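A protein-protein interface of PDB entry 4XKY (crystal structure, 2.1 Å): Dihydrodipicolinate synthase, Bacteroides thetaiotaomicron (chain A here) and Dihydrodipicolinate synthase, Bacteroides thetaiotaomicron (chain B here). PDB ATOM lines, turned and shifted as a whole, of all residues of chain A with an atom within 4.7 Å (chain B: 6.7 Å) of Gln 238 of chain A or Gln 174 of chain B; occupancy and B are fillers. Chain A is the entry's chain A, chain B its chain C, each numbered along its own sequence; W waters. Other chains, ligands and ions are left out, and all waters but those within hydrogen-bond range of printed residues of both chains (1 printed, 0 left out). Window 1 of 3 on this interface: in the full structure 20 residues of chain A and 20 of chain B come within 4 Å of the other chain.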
ATOM      1  N   GLU A 194      17.344 -33.925  15.427  1.00  0.00           N
ATOM      2  CA  GLU A 194      18.110 -32.704  15.207  1.00  0.00           C
ATOM      3  C   GLU A 194      17.411 -31.741  14.209  1.00  0.00           C
ATOM      4  O   GLU A 194      17.664 -30.550  14.211  1.00  0.00           O
ATOM      5  CB  GLU A 194      19.535 -33.053  14.759  1.00  0.00           C
ATOM      6  CG  GLU A 194      20.336 -33.851  15.808  1.00  0.00           C
ATOM      7  CD  GLU A 194      20.194 -35.349  15.669  1.00  0.00           C
ATOM      8  OE1 GLU A 194      19.263 -35.827  14.955  1.00  0.00           O
ATOM      9  OE2 GLU A 194      21.042 -36.048  16.266  1.00  0.00           O
ATOM     10  N   ILE A 195      16.497 -32.257  13.393  1.00  0.00           N
ATOM     11  CA  ILE A 195      15.830 -31.446  12.378  1.00  0.00           C
ATOM     12  C   ILE A 195      14.304 -31.413  12.543  1.00  0.00           C
ATOM     13  O   ILE A 195      13.580 -31.024  11.613  1.00  0.00           O
ATOM     14  CB  ILE A 195      16.155 -31.955  10.965  1.00  0.00           C
ATOM     15  CG1 ILE A 195      15.806 -33.443  10.817  1.00  0.00           C
ATOM     16  CG2 ILE A 195      17.604 -31.671  10.650  1.00  0.00           C
ATOM     17  CD1 ILE A 195      15.797 -33.945   9.383  1.00  0.00           C
ATOM     18  N   ALA A 197      12.609 -29.513  14.746  1.00  0.00           N
ATOM     19  CA  ALA A 197      12.166 -28.133  14.901  1.00  0.00           C
ATOM     20  C   ALA A 197      12.072 -27.444  13.545  1.00  0.00           C
ATOM     21  O   ALA A 197      11.086 -26.769  13.250  1.00  0.00           O
ATOM     22  CB  ALA A 197      13.097 -27.363  15.818  1.00  0.00           C
ATOM     23  N   GLU A 198      13.075 -27.636  12.694  1.00  0.00           N
ATOM     24  CA  GLU A 198      13.049 -26.913  11.440  1.00  0.00           C
ATOM     25  C   GLU A 198      11.972 -27.498  10.511  1.00  0.00           C
ATOM     26  O   GLU A 198      11.310 -26.761   9.791  1.00  0.00           O
ATOM     27  CB  GLU A 198      14.431 -26.859  10.806  1.00  0.00           C
ATOM     28  CG  GLU A 198      14.840 -28.090  10.040  1.00  0.00           C
ATOM     29  CD  GLU A 198      16.319 -28.043   9.708  1.00  0.00           C
ATOM     30  OE1 GLU A 198      16.668 -28.069   8.502  1.00  0.00           O
ATOM     31  OE2 GLU A 198      17.121 -27.955  10.663  1.00  0.00           O
ATOM     32  N   LEU A 222       9.654 -28.410  22.473  1.00  0.00           N
ATOM     33  CA  LEU A 222      10.250 -27.919  21.245  1.00  0.00           C
ATOM     34  C   LEU A 222       9.271 -28.046  20.075  1.00  0.00           C
ATOM     35  O   LEU A 222       9.147 -27.119  19.251  1.00  0.00           O
ATOM     36  CB  LEU A 222      11.571 -28.615  20.954  1.00  0.00           C
ATOM     37  CG  LEU A 222      12.330 -28.263  19.668  1.00  0.00           C
ATOM     38  CD1 LEU A 222      12.443 -26.775  19.354  1.00  0.00           C
ATOM     39  CD2 LEU A 222      13.721 -28.866  19.789  1.00  0.00           C
ATOM     40  N   GLU A 233      12.186 -19.521  22.014  1.00  0.00           N
ATOM     41  CA  GLU A 233      12.052 -20.838  22.621  1.00  0.00           C
ATOM     42  C   GLU A 233      12.544 -21.972  21.685  1.00  0.00           C
ATOM     43  O   GLU A 233      13.209 -22.921  22.142  1.00  0.00           O
ATOM     44  CB  GLU A 233      10.601 -21.040  23.061  1.00  0.00           C
ATOM     45  CG  GLU A 233      10.397 -22.056  24.169  1.00  0.00           C
ATOM     46  CD  GLU A 233      11.023 -21.674  25.503  1.00  0.00           C
ATOM     47  OE1 GLU A 233      11.689 -20.621  25.657  1.00  0.00           O
ATOM     48  OE2 GLU A 233      10.859 -22.471  26.431  1.00  0.00           O
ATOM     49  N   VAL A 234      12.243 -21.891  20.389  1.00  0.00           N
ATOM     50  CA  VAL A 234      12.840 -22.846  19.426  1.00  0.00           C
ATOM     51  C   VAL A 234      14.376 -22.833  19.584  1.00  0.00           C
ATOM     52  O   VAL A 234      15.006 -23.882  19.761  1.00  0.00           O
ATOM     53  CB  VAL A 234      12.451 -22.536  17.963  1.00  0.00           C
ATOM     54  CG1 VAL A 234      13.288 -23.336  16.992  1.00  0.00           C
ATOM     55  CG2 VAL A 234      10.994 -22.846  17.718  1.00  0.00           C
ATOM     56  N   ARG A 235      14.970 -21.641  19.574  1.00  0.00           N
ATOM     57  CA  ARG A 235      16.428 -21.533  19.709  1.00  0.00           C
ATOM     58  C   ARG A 235      16.961 -22.093  21.026  1.00  0.00           C
ATOM     59  O   ARG A 235      17.956 -22.802  21.033  1.00  0.00           O
ATOM     60  CB  ARG A 235      16.911 -20.093  19.488  1.00  0.00           C
ATOM     61  CG  ARG A 235      16.955 -19.719  18.010  1.00  0.00           C
ATOM     62  CD  ARG A 235      17.543 -18.333  17.770  1.00  0.00           C
ATOM     63  NE  ARG A 235      16.732 -17.287  18.390  1.00  0.00           N
ATOM     64  CZ  ARG A 235      15.792 -16.559  17.780  1.00  0.00           C
ATOM     65  NH1 ARG A 235      15.511 -16.721  16.483  1.00  0.00           N
ATOM     66  NH2 ARG A 235      15.118 -15.649  18.483  1.00  0.00           N
ATOM     67  N   ARG A 236      16.298 -21.780  22.131  1.00  0.00           N
ATOM     68  CA  ARG A 236      16.752 -22.233  23.436  1.00  0.00           C
ATOM     69  C   ARG A 236      16.731 -23.753  23.516  1.00  0.00           C
ATOM     70  O   ARG A 236      17.695 -24.379  23.976  1.00  0.00           O
ATOM     71  CB  ARG A 236      15.846 -21.661  24.526  1.00  0.00           C
ATOM     72  CG  ARG A 236      16.384 -21.874  25.935  1.00  0.00           C
ATOM     73  CD  ARG A 236      15.552 -21.135  26.965  1.00  0.00           C
ATOM     74  NE  ARG A 236      14.223 -21.713  27.146  1.00  0.00           N
ATOM     75  CZ  ARG A 236      13.958 -22.806  27.860  1.00  0.00           C
ATOM     76  NH1 ARG A 236      14.932 -23.483  28.462  1.00  0.00           N
ATOM     77  NH2 ARG A 236      12.705 -23.226  27.977  1.00  0.00           N
ATOM     78  N   LEU A 237      15.617 -24.329  23.057  1.00  0.00           N
ATOM     79  CA  LEU A 237      15.390 -25.774  23.149  1.00  0.00           C
ATOM     80  C   LEU A 237      16.180 -26.547  22.104  1.00  0.00           C
ATOM     81  O   LEU A 237      16.656 -27.642  22.387  1.00  0.00           O
ATOM     82  CB  LEU A 237      13.899 -26.094  23.068  1.00  0.00           C
ATOM     83  CG  LEU A 237      13.089 -25.494  24.231  1.00  0.00           C
ATOM     84  CD1 LEU A 237      11.600 -25.783  24.099  1.00  0.00           C
ATOM     85  CD2 LEU A 237      13.591 -25.971  25.588  1.00  0.00           C
ATOM     86  N   GLN A 238      16.331 -25.984  20.906  1.00  0.00           N
ATOM     87  CA  GLN A 238      17.189 -26.608  19.896  1.00  0.00           C
ATOM     88  C   GLN A 238      18.630 -26.793  20.427  1.00  0.00           C
ATOM     89  O   GLN A 238      19.268 -27.819  20.159  1.00  0.00           O
ATOM     90  CB  GLN A 238      17.172 -25.813  18.573  1.00  0.00           C
ATOM     91  CG  GLN A 238      18.022 -26.398  17.449  1.00  0.00           C
ATOM     92  CD  GLN A 238      17.520 -27.753  16.960  1.00  0.00           C
ATOM     93  OE1 GLN A 238      16.491 -28.262  17.421  1.00  0.00           O
ATOM     94  NE2 GLN A 238      18.246 -28.344  16.028  1.00  0.00           N
ATOM     95  N   GLU A 239      19.133 -25.829  21.190  1.00  0.00           N
ATOM     96  CA  GLU A 239      20.494 -25.931  21.722  1.00  0.00           C
ATOM     97  C   GLU A 239      20.620 -27.115  22.677  1.00  0.00           C
ATOM     98  O   GLU A 239      21.646 -27.801  22.677  1.00  0.00           O
ATOM     99  CB  GLU A 239      20.955 -24.638  22.414  1.00  0.00           C
ATOM    100  CG  GLU A 239      22.329 -24.768  23.098  1.00  0.00           C
ATOM    101  CD  GLU A 239      23.056 -23.444  23.343  1.00  0.00           C
ATOM    102  OE1 GLU A 239      22.402 -22.383  23.405  1.00  0.00           O
ATOM    103  OE2 GLU A 239      24.301 -23.462  23.495  1.00  0.00           O
ATOM    104  N   LYS A 240      19.589 -27.352  23.485  1.00  0.00           N
ATOM    105  CA  LYS A 240      19.579 -28.509  24.380  1.00  0.00           C
ATOM    106  C   LYS A 240      19.507 -29.812  23.577  1.00  0.00           C
ATOM    107  O   LYS A 240      20.269 -30.748  23.832  1.00  0.00           O
ATOM    108  CB  LYS A 240      18.405 -28.443  25.358  1.00  0.00           C
ATOM    109  CG  LYS A 240      18.527 -27.373  26.432  1.00  0.00           C
ATOM    110  CD  LYS A 240      17.405 -27.549  27.451  1.00  0.00           C
ATOM    111  CE  LYS A 240      17.042 -26.261  28.173  1.00  0.00           C
ATOM    112  NZ  LYS A 240      18.012 -25.983  29.266  1.00  0.00           N
ATOM    113  N   VAL A 241      18.581 -29.886  22.623  1.00  0.00           N
ATOM    114  CA  VAL A 241      18.545 -31.031  21.727  1.00  0.00           C
ATOM    115  C   VAL A 241      19.902 -31.239  21.065  1.00  0.00           C
ATOM    116  O   VAL A 241      20.375 -32.370  21.010  1.00  0.00           O
ATOM    117  CB  VAL A 241      17.426 -30.922  20.680  1.00  0.00           C
ATOM    118  CG1 VAL A 241      17.559 -32.002  19.615  1.00  0.00           C
ATOM    119  CG2 VAL A 241      16.081 -31.082  21.365  1.00  0.00           C
ATOM    120  N   MET A 242      20.569 -30.178  20.601  1.00  0.00           N
ATOM    121  CA  MET A 242      21.854 -30.407  19.912  1.00  0.00           C
ATOM    122  C   MET A 242      22.962 -30.823  20.882  1.00  0.00           C
ATOM    123  O   MET A 242      23.870 -31.564  20.505  1.00  0.00           O
ATOM    124  CB  MET A 242      22.278 -29.239  19.016  1.00  0.00           C
ATOM    125  CG  MET A 242      21.403 -29.012  17.780  1.00  0.00           C
ATOM    126  SD  MET A 242      20.959 -30.458  16.773  1.00  0.00           S
ATOM    127  CE  MET A 242      22.608 -30.989  16.297  1.00  0.00           C
ATOM    128  N   ASN B 169      21.926 -32.769   3.794  1.00  0.00           N
ATOM    129  CA  ASN B 169      21.700 -33.443   5.084  1.00  0.00           C
ATOM    130  C   ASN B 169      21.730 -32.430   6.219  1.00  0.00           C
ATOM    131  O   ASN B 169      22.800 -31.905   6.563  1.00  0.00           O
ATOM    132  CB  ASN B 169      22.732 -34.538   5.316  1.00  0.00           C
ATOM    133  CG  ASN B 169      22.568 -35.219   6.659  1.00  0.00           C
ATOM    134  OD1 ASN B 169      21.977 -34.669   7.592  1.00  0.00           O
ATOM    135  ND2 ASN B 169      23.077 -36.424   6.761  1.00  0.00           N
ATOM    136  N   THR B 170      20.553 -32.132   6.768  1.00  0.00           N
ATOM    137  CA  THR B 170      20.422 -31.036   7.714  1.00  0.00           C
ATOM    138  C   THR B 170      20.730 -31.445   9.152  1.00  0.00           C
ATOM    139  O   THR B 170      21.009 -30.586   9.981  1.00  0.00           O
ATOM    140  CB  THR B 170      19.063 -30.286   7.596  1.00  0.00           C
ATOM    141  OG1 THR B 170      17.977 -31.203   7.485  1.00  0.00           O
ATOM    142  CG2 THR B 170      19.068 -29.414   6.393  1.00  0.00           C
ATOM    143  N   VAL B 171      20.720 -32.740   9.449  1.00  0.00           N
ATOM    144  CA  VAL B 171      21.244 -33.251  10.721  1.00  0.00           C
ATOM    145  C   VAL B 171      22.739 -32.930  10.793  1.00  0.00           C
ATOM    146  O   VAL B 171      23.222 -32.342  11.775  1.00  0.00           O
ATOM    147  CB  VAL B 171      21.013 -34.766  10.848  1.00  0.00           C
ATOM    148  CG1 VAL B 171      21.859 -35.374  11.963  1.00  0.00           C
ATOM    149  CG2 VAL B 171      19.516 -35.068  11.023  1.00  0.00           C
ATOM    150  N   TYR B 172      23.464 -33.321   9.746  1.00  0.00           N
ATOM    151  CA  TYR B 172      24.876 -32.927   9.573  1.00  0.00           C
ATOM    152  C   TYR B 172      25.038 -31.407   9.660  1.00  0.00           C
ATOM    153  O   TYR B 172      25.843 -30.923  10.424  1.00  0.00           O
ATOM    154  CB  TYR B 172      25.403 -33.421   8.231  1.00  0.00           C
ATOM    155  CG  TYR B 172      26.759 -32.858   7.889  1.00  0.00           C
ATOM    156  CD1 TYR B 172      27.912 -33.355   8.493  1.00  0.00           C
ATOM    157  CD2 TYR B 172      26.880 -31.820   6.978  1.00  0.00           C
ATOM    158  CE1 TYR B 172      29.148 -32.833   8.179  1.00  0.00           C
ATOM    159  CE2 TYR B 172      28.107 -31.279   6.666  1.00  0.00           C
ATOM    160  CZ  TYR B 172      29.235 -31.786   7.264  1.00  0.00           C
ATOM    161  OH  TYR B 172      30.434 -31.228   6.921  1.00  0.00           O
ATOM    162  N   PHE B 173      24.239 -30.651   8.918  1.00  0.00           N
ATOM    163  CA  PHE B 173      24.372 -29.192   8.951  1.00  0.00           C
ATOM    164  C   PHE B 173      24.178 -28.590  10.357  1.00  0.00           C
ATOM    165  O   PHE B 173      25.001 -27.783  10.800  1.00  0.00           O
ATOM    166  CB  PHE B 173      23.460 -28.517   7.924  1.00  0.00           C
ATOM    167  CG  PHE B 173      23.785 -27.063   7.714  1.00  0.00           C
ATOM    168  CD1 PHE B 173      24.858 -26.679   6.921  1.00  0.00           C
ATOM    169  CD2 PHE B 173      23.057 -26.080   8.357  1.00  0.00           C
ATOM    170  CE1 PHE B 173      25.171 -25.344   6.748  1.00  0.00           C
ATOM    171  CE2 PHE B 173      23.372 -24.750   8.190  1.00  0.00           C
ATOM    172  CZ  PHE B 173      24.430 -24.378   7.398  1.00  0.00           C
ATOM    173  N   GLN B 174      23.140 -29.019  11.079  1.00  0.00           N
ATOM    174  CA  GLN B 174      22.933 -28.576  12.468  1.00  0.00           C
ATOM    175  C   GLN B 174      24.079 -28.964  13.405  1.00  0.00           C
ATOM    176  O   GLN B 174      24.409 -28.207  14.322  1.00  0.00           O
ATOM    177  CB  GLN B 174      21.625 -29.136  13.024  1.00  0.00           C
ATOM    178  CG  GLN B 174      20.396 -28.567  12.344  1.00  0.00           C
ATOM    179  CD  GLN B 174      20.246 -27.093  12.621  1.00  0.00           C
ATOM    180  OE1 GLN B 174      20.332 -26.663  13.770  1.00  0.00           O
ATOM    181  NE2 GLN B 174      20.023 -26.306  11.575  1.00  0.00           N
ATOM    182  N   SER B 175      24.678 -30.137  13.180  1.00  0.00           N
ATOM    183  CA  SER B 175      25.842 -30.551  13.952  1.00  0.00           C
ATOM    184  C   SER B 175      27.024 -29.602  13.765  1.00  0.00           C
ATOM    185  O   SER B 175      27.779 -29.379  14.704  1.00  0.00           O
ATOM    186  CB  SER B 175      26.259 -31.968  13.598  1.00  0.00           C
ATOM    187  OG  SER B 175      25.229 -32.887  13.932  1.00  0.00           O
ATOM    188  N   VAL B 176      27.185 -29.048  12.563  1.00  0.00           N
ATOM    189  CA  VAL B 176      28.285 -28.115  12.310  1.00  0.00           C
ATOM    190  C   VAL B 176      27.923 -26.744  12.868  1.00  0.00           C
ATOM    191  O   VAL B 176      28.785 -26.063  13.395  1.00  0.00           O
ATOM    192  CB  VAL B 176      28.639 -27.990  10.801  1.00  0.00           C
ATOM    193  CG1 VAL B 176      29.859 -27.093  10.586  1.00  0.00           C
ATOM    194  CG2 VAL B 176      28.895 -29.356  10.175  1.00  0.00           C
ATOM    195  N   MET B 177      26.656 -26.339  12.771  1.00  0.00           N
ATOM    196  CA  MET B 177      26.206 -25.090  13.407  1.00  0.00           C
ATOM    197  C   MET B 177      26.522 -25.113  14.905  1.00  0.00           C
ATOM    198  O   MET B 177      27.098 -24.170  15.467  1.00  0.00           O
ATOM    199  CB  MET B 177      24.700 -24.882  13.211  1.00  0.00           C
ATOM    200  CG  MET B 177      24.269 -24.500  11.790  1.00  0.00           C
ATOM    201  SD  MET B 177      24.679 -22.809  11.280  1.00  0.00           S
ATOM    202  CE  MET B 177      23.666 -21.970  12.508  1.00  0.00           C
ATOM    203  N   TYR B 178      26.148 -26.207  15.550  1.00  0.00           N
ATOM    204  CA  TYR B 178      26.388 -26.371  16.979  1.00  0.00           C
ATOM    205  C   TYR B 178      27.896 -26.292  17.293  1.00  0.00           C
ATOM    206  O   TYR B 178      28.295 -25.618  18.224  1.00  0.00           O
ATOM    207  CB  TYR B 178      25.778 -27.683  17.487  1.00  0.00           C
ATOM    208  CG  TYR B 178      25.951 -27.882  18.980  1.00  0.00           C
ATOM    209  CD1 TYR B 178      25.083 -27.281  19.881  1.00  0.00           C
ATOM    210  CD2 TYR B 178      27.015 -28.631  19.486  1.00  0.00           C
ATOM    211  CE1 TYR B 178      25.247 -27.446  21.252  1.00  0.00           C
ATOM    212  CE2 TYR B 178      27.187 -28.801  20.854  1.00  0.00           C
ATOM    213  CZ  TYR B 178      26.297 -28.203  21.725  1.00  0.00           C
ATOM    214  OH  TYR B 178      26.433 -28.349  23.070  1.00  0.00           O
ATOM    215  N   ALA B 179      28.724 -26.948  16.487  1.00  0.00           N
ATOM    216  CA  ALA B 179      30.159 -26.915  16.690  1.00  0.00           C
ATOM    217  C   ALA B 179      30.730 -25.509  16.493  1.00  0.00           C
ATOM    218  O   ALA B 179      31.723 -25.165  17.114  1.00  0.00           O
ATOM    219  CB  ALA B 179      30.841 -27.893  15.751  1.00  0.00           C
ATOM    220  N   MET B 188      28.159 -19.598   7.561  1.00  0.00           N
ATOM    221  CA  MET B 188      27.572 -20.925   7.397  1.00  0.00           C
ATOM    222  C   MET B 188      26.523 -20.828   6.302  1.00  0.00           C
ATOM    223  O   MET B 188      25.462 -20.219   6.486  1.00  0.00           O
ATOM    224  CB  MET B 188      26.920 -21.395   8.709  1.00  0.00           C
ATOM    225  CG  MET B 188      27.891 -21.708   9.836  1.00  0.00           C
ATOM    226  SD  MET B 188      28.855 -23.200   9.508  1.00  0.00           S
ATOM    227  CE  MET B 188      27.603 -24.474   9.569  1.00  0.00           C
ATOM    228  N   GLU B 198      14.428 -23.043   5.874  1.00  0.00           N
ATOM    229  CA  GLU B 198      14.426 -23.688   7.181  1.00  0.00           C
ATOM    230  C   GLU B 198      15.771 -23.545   7.856  1.00  0.00           C
ATOM    231  O   GLU B 198      15.821 -23.438   9.067  1.00  0.00           O
ATOM    232  CB  GLU B 198      13.996 -25.160   7.131  1.00  0.00           C
ATOM    233  CG  GLU B 198      15.008 -26.135   6.565  1.00  0.00           C
ATOM    234  CD  GLU B 198      14.391 -27.483   6.228  1.00  0.00           C
ATOM    235  OE1 GLU B 198      14.777 -28.479   6.852  1.00  0.00           O
ATOM    236  OE2 GLU B 198      13.535 -27.560   5.330  1.00  0.00           O
ATOM    237  N   SER B 199      16.851 -23.547   7.077  1.00  0.00           N
ATOM    238  CA  SER B 199      18.200 -23.400   7.640  1.00  0.00           C
ATOM    239  C   SER B 199      18.443 -21.989   8.130  1.00  0.00           C
ATOM    240  O   SER B 199      19.022 -21.785   9.206  1.00  0.00           O
ATOM    241  CB  SER B 199      19.262 -23.747   6.605  1.00  0.00           C
ATOM    242  OG  SER B 199      19.025 -25.036   6.063  1.00  0.00           O
ATOM    243  N   LEU B 202      16.866 -21.167  11.431  1.00  0.00           N
ATOM    244  CA  LEU B 202      17.684 -21.691  12.514  1.00  0.00           C
ATOM    245  C   LEU B 202      19.106 -21.154  12.493  1.00  0.00           C
ATOM    246  O   LEU B 202      20.014 -21.793  13.011  1.00  0.00           O
ATOM    247  CB  LEU B 202      17.706 -23.219  12.438  1.00  0.00           C
ATOM    248  CG  LEU B 202      16.617 -23.891  13.276  1.00  0.00           C
ATOM    249  CD1 LEU B 202      15.211 -23.573  12.803  1.00  0.00           C
ATOM    250  CD2 LEU B 202      16.849 -25.373  13.206  1.00  0.00           C
ATOM    251  N   GLY B 203      19.305 -20.001  11.863  1.00  0.00           N
ATOM    252  CA  GLY B 203      20.537 -19.241  12.031  1.00  0.00           C
ATOM    253  C   GLY B 203      21.599 -19.381  10.963  1.00  0.00           C
ATOM    254  O   GLY B 203      22.667 -18.797  11.097  1.00  0.00           O
ATOM    255  N   ALA B 204      21.332 -20.139   9.901  1.00  0.00           N
ATOM    256  CA  ALA B 204      22.267 -20.187   8.787  1.00  0.00           C
ATOM    257  C   ALA B 204      22.352 -18.778   8.205  1.00  0.00           C
ATOM    258  O   ALA B 204      21.347 -18.067   8.147  1.00  0.00           O
ATOM    259  CB  ALA B 204      21.793 -21.170   7.725  1.00  0.00           C
HETATM  260  O   HOH W   1      19.492 -27.064   8.980  1.00  0.00           O
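OE1 of Glu 198 of chain A sits close to OE1 of Glu 198 of chain B, at 2.5 Å.
The side-chain carboxylate of Glu 198 of chain A sits at hydrogen-bond distance from the side-chain amide nitrogen of Gln 174 of chain B (3.5 Å).
The backbone carbonyl oxygen (O) of Val 171 of chain B sits at hydrogen-bond distance from the side-chain hydroxyl (OG) of Ser 175 of chain B (3.0 Å).
The backbone carbonyl oxygen of Glu 194 of chain A is in hydrogen-bond range of the side-chain amide nitrogen of Gln 238 of chain A, at 2.9 Å.
N of Val 171 of chain B sits at hydrogen-bond distance from OD1 of Asn 169 of chain B, at 3.0 Å.
The side-chain amide nitrogen (NE2) of Gln 238 of chain A sits at hydrogen-bond distance from the side-chain sulfur (SD) of Met 242 of chain A, 3.5 Å away.
OE1 of Glu 194 of chain A touches CG1 of Val 171 of chain B, at 3.99 Å.
O of Glu 194 of chain A touches CG of Gln 174 of chain B, 3.9 Å away.
OG1 of Thr 170 of chain B touches CG2 of Ile 195 of chain A (3.2 Å).
Ile 195 of chain A touches Val 171 of chain B (CG2 to N, 3.5 Å).
Glu 198 of chain A touches Leu 202 of chain B (OE2 to CD2, 3.6 Å).
NE2 of Gln 238 of chain A touches OE1 of Gln 174 of chain B, at 3.5 Å.
O of Glu 239 of chain A touches CE1 of Tyr 178 of chain B (3.9 Å).
C of Gln 174 of chain B touches CE of Met 242 of chain A (3.8 Å).
Ser 175 of chain B touches Met 242 of chain A.
Tyr 178 of chain B touches Met 242 of chain A.
Of the printed residues of chain B, Ile 195 of chain A touches Thr 170 (3.2 Å) and Val 171 (3.5 Å).
Of chain B, only Gln 174 (3.5 Å) comes within 4 Å of Gln 238 of chain A.
Printed residues of chain A within 4 Å of Val 171 of chain B: Glu 194 (3.99 Å) and Ile 195 (3.5 Å).
The nearest residue of chain B that does not touch Gln 238 of chain A is Leu 202 of chain B (4.3 Å).
Of the 17 printed residues of chain B, 7 touch a printed residue of chain A.
Printed residues of chain B that touch a printed residue of chain A: Thr 170, Val 171, Gln 174, Ser 175, Tyr 178, Glu 198 and Leu 202.
Hydrophobic or aromatic side chains of chain B that line the printed part of chain A: Val 171, Tyr 178 and Leu 202.
Of the 15 printed residues of chain A, 6 touch a printed residue of chain B.
Hydrophobic or aromatic side chains of chain A that line the printed part of chain B: Ile 195 and Met 242.
Among the printed residues, no Asp or Glu carboxylate lies within 4 Å of a Lys or Arg side-chain nitrogen of the other chain.
Water W1 lies within hydrogen-bond range of NE2 of Gln 174 of chain B and OE1 of Glu 198 of chain A.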
